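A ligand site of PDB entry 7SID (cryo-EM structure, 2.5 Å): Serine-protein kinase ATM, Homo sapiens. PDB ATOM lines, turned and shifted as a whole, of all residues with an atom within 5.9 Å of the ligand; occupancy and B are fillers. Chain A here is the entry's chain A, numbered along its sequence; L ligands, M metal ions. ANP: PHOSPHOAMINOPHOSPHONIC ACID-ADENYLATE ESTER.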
ATOM      1  N   ALA A2693       0.147   5.277 -29.682  1.00  0.00           N
ATOM      2  CA  ALA A2693      -0.527   6.048 -28.653  1.00  0.00           C
ATOM      3  C   ALA A2693       0.048   5.670 -27.291  1.00  0.00           C
ATOM      4  O   ALA A2693       0.174   4.489 -26.982  1.00  0.00           O
ATOM      5  CB  ALA A2693      -2.034   5.818 -28.679  1.00  0.00           C
ATOM      6  N   GLY A2694       0.397   6.676 -26.500  1.00  0.00           N
ATOM      7  CA  GLY A2694       0.996   6.445 -25.200  1.00  0.00           C
ATOM      8  C   GLY A2694       0.123   5.628 -24.265  1.00  0.00           C
ATOM      9  O   GLY A2694      -1.008   6.029 -23.950  1.00  0.00           O
ATOM     10  N   GLY A2695       0.637   4.495 -23.819  1.00  0.00           N
ATOM     11  CA  GLY A2695      -0.125   3.618 -22.939  1.00  0.00           C
ATOM     12  C   GLY A2695       0.650   2.351 -22.676  1.00  0.00           C
ATOM     13  O   GLY A2695       1.680   2.073 -23.312  1.00  0.00           O
ATOM     14  N   VAL A2696       0.143   1.579 -21.712  1.00  0.00           N
ATOM     15  CA  VAL A2696       0.800   0.328 -21.337  1.00  0.00           C
ATOM     16  C   VAL A2696       0.659  -0.710 -22.437  1.00  0.00           C
ATOM     17  O   VAL A2696       1.614  -1.404 -22.783  1.00  0.00           O
ATOM     18  CB  VAL A2696       0.249  -0.180 -19.994  1.00  0.00           C
ATOM     19  CG1 VAL A2696       0.913  -1.490 -19.604  1.00  0.00           C
ATOM     20  CG2 VAL A2696       0.429   0.869 -18.913  1.00  0.00           C
ATOM     21  N   ASN A2697      -0.531  -0.819 -23.024  1.00  0.00           N
ATOM     22  CA  ASN A2697      -0.805  -1.830 -24.037  1.00  0.00           C
ATOM     23  C   ASN A2697      -0.420  -1.389 -25.442  1.00  0.00           C
ATOM     24  O   ASN A2697      -0.472  -2.219 -26.368  1.00  0.00           O
ATOM     25  CB  ASN A2697      -2.287  -2.224 -24.012  1.00  0.00           C
ATOM     26  CG  ASN A2697      -2.600  -3.259 -22.944  1.00  0.00           C
ATOM     27  OD1 ASN A2697      -2.127  -4.392 -23.009  1.00  0.00           O
ATOM     28  ND2 ASN A2697      -3.385  -2.866 -21.948  1.00  0.00           N
ATOM     29  N   PRO A2699      -1.731   0.943 -27.978  1.00  0.00           N
ATOM     30  CA  PRO A2699      -2.680   0.880 -29.101  1.00  0.00           C
ATOM     31  C   PRO A2699      -2.073   1.485 -30.355  1.00  0.00           C
ATOM     32  O   PRO A2699      -1.179   2.339 -30.290  1.00  0.00           O
ATOM     33  CB  PRO A2699      -3.877   1.705 -28.610  1.00  0.00           C
ATOM     34  CG  PRO A2699      -3.682   1.851 -27.128  1.00  0.00           C
ATOM     35  CD  PRO A2699      -2.200   1.854 -26.916  1.00  0.00           C
ATOM     36  N   LEU A2715      -8.006   3.998 -34.214  1.00  0.00           N
ATOM     37  CA  LEU A2715      -7.219   3.407 -33.142  1.00  0.00           C
ATOM     38  C   LEU A2715      -7.586   1.942 -33.019  1.00  0.00           C
ATOM     39  O   LEU A2715      -8.726   1.602 -32.674  1.00  0.00           O
ATOM     40  CB  LEU A2715      -7.462   4.139 -31.816  1.00  0.00           C
ATOM     41  CG  LEU A2715      -6.553   3.739 -30.648  1.00  0.00           C
ATOM     42  CD1 LEU A2715      -5.157   4.284 -30.863  1.00  0.00           C
ATOM     43  CD2 LEU A2715      -7.132   4.214 -29.325  1.00  0.00           C
ATOM     44  N   LYS A2717      -7.127  -1.436 -31.025  1.00  0.00           N
ATOM     45  CA  LYS A2717      -6.823  -1.839 -29.665  1.00  0.00           C
ATOM     46  C   LYS A2717      -6.911  -3.355 -29.549  1.00  0.00           C
ATOM     47  O   LYS A2717      -7.800  -3.980 -30.152  1.00  0.00           O
ATOM     48  CB  LYS A2717      -7.793  -1.207 -28.665  1.00  0.00           C
ATOM     49  CG  LYS A2717      -7.422   0.196 -28.208  1.00  0.00           C
ATOM     50  CD  LYS A2717      -8.539   0.779 -27.356  1.00  0.00           C
ATOM     51  CE  LYS A2717      -7.982   1.658 -26.248  1.00  0.00           C
ATOM     52  NZ  LYS A2717      -9.018   1.965 -25.217  1.00  0.00           N
ATOM     53  N   ASP A2720      -8.364  -5.964 -24.721  1.00  0.00           N
ATOM     54  CA  ASP A2720      -9.279  -5.192 -23.900  1.00  0.00           C
ATOM     55  C   ASP A2720     -10.700  -5.392 -24.421  1.00  0.00           C
ATOM     56  O   ASP A2720     -10.900  -5.846 -25.551  1.00  0.00           O
ATOM     57  CB  ASP A2720      -8.908  -3.700 -23.878  1.00  0.00           C
ATOM     58  CG  ASP A2720      -8.825  -3.092 -25.260  1.00  0.00           C
ATOM     59  OD1 ASP A2720      -8.534  -1.878 -25.357  1.00  0.00           O
ATOM     60  OD2 ASP A2720      -9.043  -3.814 -26.251  1.00  0.00           O
ATOM     61  N   TYR A2755     -17.973   9.280 -29.952  1.00  0.00           N
ATOM     62  CA  TYR A2755     -17.107   8.685 -30.957  1.00  0.00           C
ATOM     63  C   TYR A2755     -17.552   7.252 -31.204  1.00  0.00           C
ATOM     64  O   TYR A2755     -18.266   6.648 -30.399  1.00  0.00           O
ATOM     65  CB  TYR A2755     -15.631   8.726 -30.542  1.00  0.00           C
ATOM     66  CG  TYR A2755     -15.317   8.052 -29.227  1.00  0.00           C
ATOM     67  CD1 TYR A2755     -15.560   8.688 -28.023  1.00  0.00           C
ATOM     68  CD2 TYR A2755     -14.773   6.774 -29.191  1.00  0.00           C
ATOM     69  CE1 TYR A2755     -15.280   8.075 -26.810  1.00  0.00           C
ATOM     70  CE2 TYR A2755     -14.491   6.147 -27.990  1.00  0.00           C
ATOM     71  CZ  TYR A2755     -14.745   6.807 -26.806  1.00  0.00           C
ATOM     72  OH  TYR A2755     -14.456   6.182 -25.612  1.00  0.00           O
ATOM     73  N   LEU A2767     -11.616   1.770 -32.898  1.00  0.00           N
ATOM     74  CA  LEU A2767     -12.425   2.924 -32.551  1.00  0.00           C
ATOM     75  C   LEU A2767     -11.961   4.139 -33.345  1.00  0.00           C
ATOM     76  O   LEU A2767     -10.883   4.150 -33.951  1.00  0.00           O
ATOM     77  CB  LEU A2767     -12.382   3.195 -31.043  1.00  0.00           C
ATOM     78  CG  LEU A2767     -11.068   3.523 -30.331  1.00  0.00           C
ATOM     79  CD1 LEU A2767     -10.700   4.993 -30.441  1.00  0.00           C
ATOM     80  CD2 LEU A2767     -11.139   3.094 -28.864  1.00  0.00           C
ATOM     81  N   GLU A2768     -12.809   5.167 -33.358  1.00  0.00           N
ATOM     82  CA  GLU A2768     -12.532   6.380 -34.099  1.00  0.00           C
ATOM     83  C   GLU A2768     -11.621   7.296 -33.282  1.00  0.00           C
ATOM     84  O   GLU A2768     -11.901   7.581 -32.113  1.00  0.00           O
ATOM     85  CB  GLU A2768     -13.834   7.100 -34.447  1.00  0.00           C
ATOM     86  CG  GLU A2768     -13.654   8.530 -34.918  1.00  0.00           C
ATOM     87  CD  GLU A2768     -14.972   9.278 -35.045  1.00  0.00           C
ATOM     88  OE1 GLU A2768     -15.879   8.757 -35.733  1.00  0.00           O
ATOM     89  OE2 GLU A2768     -15.092  10.367 -34.451  1.00  0.00           O
ATOM     90  N   TRP A2769     -10.548   7.761 -33.906  1.00  0.00           N
ATOM     91  CA  TRP A2769      -9.602   8.660 -33.255  1.00  0.00           C
ATOM     92  C   TRP A2769     -10.081  10.094 -33.424  1.00  0.00           C
ATOM     93  O   TRP A2769     -10.317  10.549 -34.545  1.00  0.00           O
ATOM     94  CB  TRP A2769      -8.199   8.479 -33.840  1.00  0.00           C
ATOM     95  CG  TRP A2769      -7.154   9.347 -33.201  1.00  0.00           C
ATOM     96  CD1 TRP A2769      -6.806  10.613 -33.570  1.00  0.00           C
ATOM     97  CD2 TRP A2769      -6.333   9.013 -32.075  1.00  0.00           C
ATOM     98  NE1 TRP A2769      -5.810  11.080 -32.748  1.00  0.00           N
ATOM     99  CE2 TRP A2769      -5.499  10.121 -31.826  1.00  0.00           C
ATOM    100  CE3 TRP A2769      -6.212   7.878 -31.265  1.00  0.00           C
ATOM    101  CZ2 TRP A2769      -4.561  10.136 -30.792  1.00  0.00           C
ATOM    102  CZ3 TRP A2769      -5.285   7.899 -30.239  1.00  0.00           C
ATOM    103  CH2 TRP A2769      -4.472   9.013 -30.020  1.00  0.00           C
ATOM    104  N   CYS A2770     -10.215  10.815 -32.306  1.00  0.00           N
ATOM    105  CA  CYS A2770     -10.697  12.186 -32.326  1.00  0.00           C
ATOM    106  C   CYS A2770      -9.552  13.100 -32.751  1.00  0.00           C
ATOM    107  O   CYS A2770      -8.626  13.355 -31.971  1.00  0.00           O
ATOM    108  CB  CYS A2770     -11.250  12.582 -30.961  1.00  0.00           C
ATOM    109  SG  CYS A2770     -12.382  11.373 -30.245  1.00  0.00           S
ATOM    110  N   THR A2771      -9.616  13.605 -33.974  1.00  0.00           N
ATOM    111  CA  THR A2771      -8.570  14.477 -34.508  1.00  0.00           C
ATOM    112  C   THR A2771      -8.746  15.899 -33.992  1.00  0.00           C
ATOM    113  O   THR A2771      -9.865  16.395 -33.843  1.00  0.00           O
ATOM    114  CB  THR A2771      -8.591  14.463 -36.035  1.00  0.00           C
ATOM    115  OG1 THR A2771      -8.619  13.107 -36.506  1.00  0.00           O
ATOM    116  CG2 THR A2771      -7.347  15.138 -36.599  1.00  0.00           C
ATOM    117  N   THR A2773      -7.812  16.963 -30.982  1.00  0.00           N
ATOM    118  CA  THR A2773      -8.067  16.969 -29.564  1.00  0.00           C
ATOM    119  C   THR A2773      -6.787  16.640 -28.799  1.00  0.00           C
ATOM    120  O   THR A2773      -5.901  15.943 -29.316  1.00  0.00           O
ATOM    121  CB  THR A2773      -9.154  15.958 -29.174  1.00  0.00           C
ATOM    122  OG1 THR A2773      -8.737  14.642 -29.539  1.00  0.00           O
ATOM    123  CG2 THR A2773     -10.455  16.283 -29.878  1.00  0.00           C
ATOM    124  N   PRO A2775      -5.485  15.591 -24.612  1.00  0.00           N
ATOM    125  CA  PRO A2775      -5.866  15.379 -23.218  1.00  0.00           C
ATOM    126  C   PRO A2775      -5.559  16.602 -22.372  1.00  0.00           C
ATOM    127  O   PRO A2775      -4.552  17.280 -22.574  1.00  0.00           O
ATOM    128  CB  PRO A2775      -5.025  14.168 -22.782  1.00  0.00           C
ATOM    129  CG  PRO A2775      -3.993  13.993 -23.848  1.00  0.00           C
ATOM    130  CD  PRO A2775      -4.586  14.531 -25.113  1.00  0.00           C
ATOM    131  N   GLN A2874      -6.219  12.099 -17.803  1.00  0.00           N
ATOM    132  CA  GLN A2874      -5.888  11.411 -19.043  1.00  0.00           C
ATOM    133  C   GLN A2874      -7.101  10.798 -19.728  1.00  0.00           C
ATOM    134  O   GLN A2874      -6.981  10.310 -20.856  1.00  0.00           O
ATOM    135  CB  GLN A2874      -4.851  10.307 -18.777  1.00  0.00           C
ATOM    136  CG  GLN A2874      -3.447  10.831 -18.561  1.00  0.00           C
ATOM    137  CD  GLN A2874      -2.902  11.542 -19.782  1.00  0.00           C
ATOM    138  OE1 GLN A2874      -2.965  11.023 -20.893  1.00  0.00           O
ATOM    139  NE2 GLN A2874      -2.350  12.731 -19.577  1.00  0.00           N
ATOM    140  N   ASN A2875      -8.282  10.812 -19.087  1.00  0.00           N
ATOM    141  CA  ASN A2875      -9.490  10.251 -19.661  1.00  0.00           C
ATOM    142  C   ASN A2875     -10.414  11.319 -20.238  1.00  0.00           C
ATOM    143  O   ASN A2875     -11.494  10.989 -20.734  1.00  0.00           O
ATOM    144  CB  ASN A2875     -10.240   9.431 -18.614  1.00  0.00           C
ATOM    145  CG  ASN A2875      -9.766   7.990 -18.553  1.00  0.00           C
ATOM    146  OD1 ASN A2875      -8.974   7.552 -19.391  1.00  0.00           O
ATOM    147  ND2 ASN A2875     -10.252   7.253 -17.570  1.00  0.00           N
ATOM    148  N   LEU A2877     -10.547  14.646 -22.923  1.00  0.00           N
ATOM    149  CA  LEU A2877      -9.878  15.362 -24.004  1.00  0.00           C
ATOM    150  C   LEU A2877     -10.606  16.669 -24.266  1.00  0.00           C
ATOM    151  O   LEU A2877     -11.805  16.800 -24.007  1.00  0.00           O
ATOM    152  CB  LEU A2877      -9.840  14.521 -25.283  1.00  0.00           C
ATOM    153  CG  LEU A2877      -9.582  13.022 -25.130  1.00  0.00           C
ATOM    154  CD1 LEU A2877      -9.812  12.311 -26.453  1.00  0.00           C
ATOM    155  CD2 LEU A2877      -8.173  12.766 -24.618  1.00  0.00           C
ATOM    156  N   ILE A2888     -13.648   9.670 -22.583  1.00  0.00           N
ATOM    157  CA  ILE A2888     -13.247   8.367 -23.090  1.00  0.00           C
ATOM    158  C   ILE A2888     -13.010   7.447 -21.904  1.00  0.00           C
ATOM    159  O   ILE A2888     -12.986   7.874 -20.751  1.00  0.00           O
ATOM    160  CB  ILE A2888     -11.996   8.436 -23.991  1.00  0.00           C
ATOM    161  CG1 ILE A2888     -10.786   8.893 -23.176  1.00  0.00           C
ATOM    162  CG2 ILE A2888     -12.239   9.378 -25.169  1.00  0.00           C
ATOM    163  CD1 ILE A2888      -9.510   8.973 -23.979  1.00  0.00           C
ATOM    164  N   ASP A2889     -12.814   6.160 -22.215  1.00  0.00           N
ATOM    165  CA  ASP A2889     -12.533   5.121 -21.218  1.00  0.00           C
ATOM    166  C   ASP A2889     -13.651   5.052 -20.170  1.00  0.00           C
ATOM    167  O   ASP A2889     -13.462   5.341 -18.982  1.00  0.00           O
ATOM    168  CB  ASP A2889     -11.162   5.348 -20.555  1.00  0.00           C
ATOM    169  CG  ASP A2889     -10.570   4.074 -20.002  1.00  0.00           C
ATOM    170  OD1 ASP A2889     -11.093   2.981 -20.307  1.00  0.00           O
ATOM    171  OD2 ASP A2889      -9.569   4.161 -19.262  1.00  0.00           O
ATOM    172  N   TYR A2969      -6.346  -3.615 -10.633  1.00  0.00           N
ATOM    173  CA  TYR A2969      -5.706  -3.010 -11.808  1.00  0.00           C
ATOM    174  C   TYR A2969      -5.953  -1.508 -11.874  1.00  0.00           C
ATOM    175  O   TYR A2969      -5.078  -0.745 -12.282  1.00  0.00           O
ATOM    176  CB  TYR A2969      -6.210  -3.691 -13.081  1.00  0.00           C
ATOM    177  CG  TYR A2969      -5.695  -3.048 -14.355  1.00  0.00           C
ATOM    178  CD1 TYR A2969      -4.395  -3.260 -14.780  1.00  0.00           C
ATOM    179  CD2 TYR A2969      -6.516  -2.229 -15.119  1.00  0.00           C
ATOM    180  CE1 TYR A2969      -3.921  -2.668 -15.936  1.00  0.00           C
ATOM    181  CE2 TYR A2969      -6.049  -1.642 -16.281  1.00  0.00           C
ATOM    182  CZ  TYR A2969      -4.751  -1.860 -16.683  1.00  0.00           C
ATOM    183  OH  TYR A2969      -4.291  -1.273 -17.837  1.00  0.00           O
HETATM  184  PG  ANP L   1      -6.814   1.510 -20.573  1.00  0.00           P
HETATM  185  O1G ANP L   1      -8.254   1.276 -20.234  1.00  0.00           O
HETATM  186  O2G ANP L   1      -5.899   0.845 -19.466  1.00  0.00           O
HETATM  187  O3G ANP L   1      -6.494   0.854 -21.974  1.00  0.00           O
HETATM  188  PB  ANP L   1      -4.939   3.423 -21.162  1.00  0.00           P
HETATM  189  O1B ANP L   1      -4.029   2.412 -20.556  1.00  0.00           O
HETATM  190  O2B ANP L   1      -4.473   4.857 -20.769  1.00  0.00           O
HETATM  191  N3B ANP L   1      -6.514   3.170 -20.650  1.00  0.00           N
HETATM  192  PA  ANP L   1      -5.888   4.126 -23.611  1.00  0.00           P
HETATM  193  O1A ANP L   1      -7.260   4.115 -23.049  1.00  0.00           O
HETATM  194  O2A ANP L   1      -5.782   3.561 -25.026  1.00  0.00           O
HETATM  195  O3A ANP L   1      -4.901   3.271 -22.713  1.00  0.00           O
HETATM  196  O5' ANP L   1      -5.342   5.606 -23.549  1.00  0.00           O
HETATM  197  C5' ANP L   1      -4.168   5.970 -24.291  1.00  0.00           C
HETATM  198  C4' ANP L   1      -4.304   7.409 -24.734  1.00  0.00           C
HETATM  199  O4' ANP L   1      -4.808   7.458 -26.071  1.00  0.00           O
HETATM  200  C3' ANP L   1      -5.285   8.244 -23.912  1.00  0.00           C
HETATM  201  O3' ANP L   1      -4.666   8.765 -22.749  1.00  0.00           O
HETATM  202  C2' ANP L   1      -5.662   9.347 -24.906  1.00  0.00           C
HETATM  203  O2' ANP L   1      -4.734  10.426 -24.867  1.00  0.00           O
HETATM  204  C1' ANP L   1      -5.593   8.631 -26.257  1.00  0.00           C
HETATM  205  N9  ANP L   1      -6.892   8.243 -26.793  1.00  0.00           N
HETATM  206  C8  ANP L   1      -7.640   7.155 -26.429  1.00  0.00           C
HETATM  207  N7  ANP L   1      -8.773   7.054 -27.071  1.00  0.00           N
HETATM  208  C5  ANP L   1      -8.779   8.145 -27.919  1.00  0.00           C
HETATM  209  C6  ANP L   1      -9.698   8.618 -28.872  1.00  0.00           C
HETATM  210  N6  ANP L   1     -10.865   8.015 -29.144  1.00  0.00           N
HETATM  211  N1  ANP L   1      -9.392   9.749 -29.541  1.00  0.00           N
HETATM  212  C2  ANP L   1      -8.235  10.357 -29.277  1.00  0.00           C
HETATM  213  N3  ANP L   1      -7.280  10.010 -28.404  1.00  0.00           N
HETATM  214  C4  ANP L   1      -7.617   8.894 -27.759  1.00  0.00           C
HETATM  215 MG    MG M   1      -7.454   5.873 -20.183  1.00  0.00          MG
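N of Cys 2770 lies within hydrogen-bond range of N1 of the ligand, at 3.1 Å. A nitrogen (N1) of the ligand sits at hydrogen-bond distance from the side-chain sulfur (SG) of Cys 2770 (3.5 Å). O2G of the ligand sits at hydrogen-bond distance from OH of Tyr 2969, 3.1 Å away. NZ of Lys 2717 lies within salt-bridge range of O1A of the ligand, at 3.5 Å. The backbone carbonyl oxygen of Glu 2768 lies within hydrogen-bond range of a nitrogen (N6) of the ligand, at 3.2 Å. A nitrogen (N3B) of the ligand sits at hydrogen-bond distance from the side-chain carboxylate of Asp 2889, at 3.5 Å. An oxygen (O3') of the ligand is in hydrogen-bond range of the backbone carbonyl oxygen of Gln 2874 (3.4 Å). An oxygen (O3') of the ligand sits at hydrogen-bond distance from the side-chain amide oxygen (OE1) of Gln 2874 (3.4 Å).
The backbone carbonyl oxygen (O) of Cys 2770 sits at hydrogen-bond distance from the side-chain hydroxyl (OG1) of Thr 2773 (2.8 Å). The side-chain carboxylate of Asp 2720 is in salt-bridge range of the side-chain amino group of Lys 2717, 3.9 Å away. O of Leu 2767 is in hydrogen-bond range of N of Leu 2715. The side-chain carboxylate (OD2) of Asp 2889 lies close to the side-chain amide oxygen (OD1) of Asn 2875 (3.4 Å). The backbone carbonyl oxygen of Pro 2699 is in hydrogen-bond range of the backbone NH of Ala 2693, 3.3 Å away. The backbone NH of Ile 2888 is in hydrogen-bond range of the backbone carbonyl oxygen of Asn 2875, at 3.1 Å.
Gly 2694 touches the ligand. CG of Pro 2699 touches O2A of the ligand (3.4 Å). Leu 2715 touches the ligand. Leu 2767 touches the ligand. Trp 2769 touches the ligand. CG of Pro 2775 touches O2' of the ligand (3.8 Å). CD1 of Leu 2877 touches C2 of the ligand (3.8 Å). Ile 2888 touches the ligand. Hydrophobic or aromatic side chains that line the ligand: Pro 2699, Leu 2715, Leu 2767, Trp 2769, Pro 2775, Leu 2877 and Ile 2888. Within 4 Å of the ligand: Gly 2694, Pro 2699, Leu 2715, Lys 2717, Leu 2767, Glu 2768, Trp 2769, Cys 2770, Pro 2775, Gln 2874, Leu 2877, Ile 2888, Asp 2889 and Tyr 2969.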
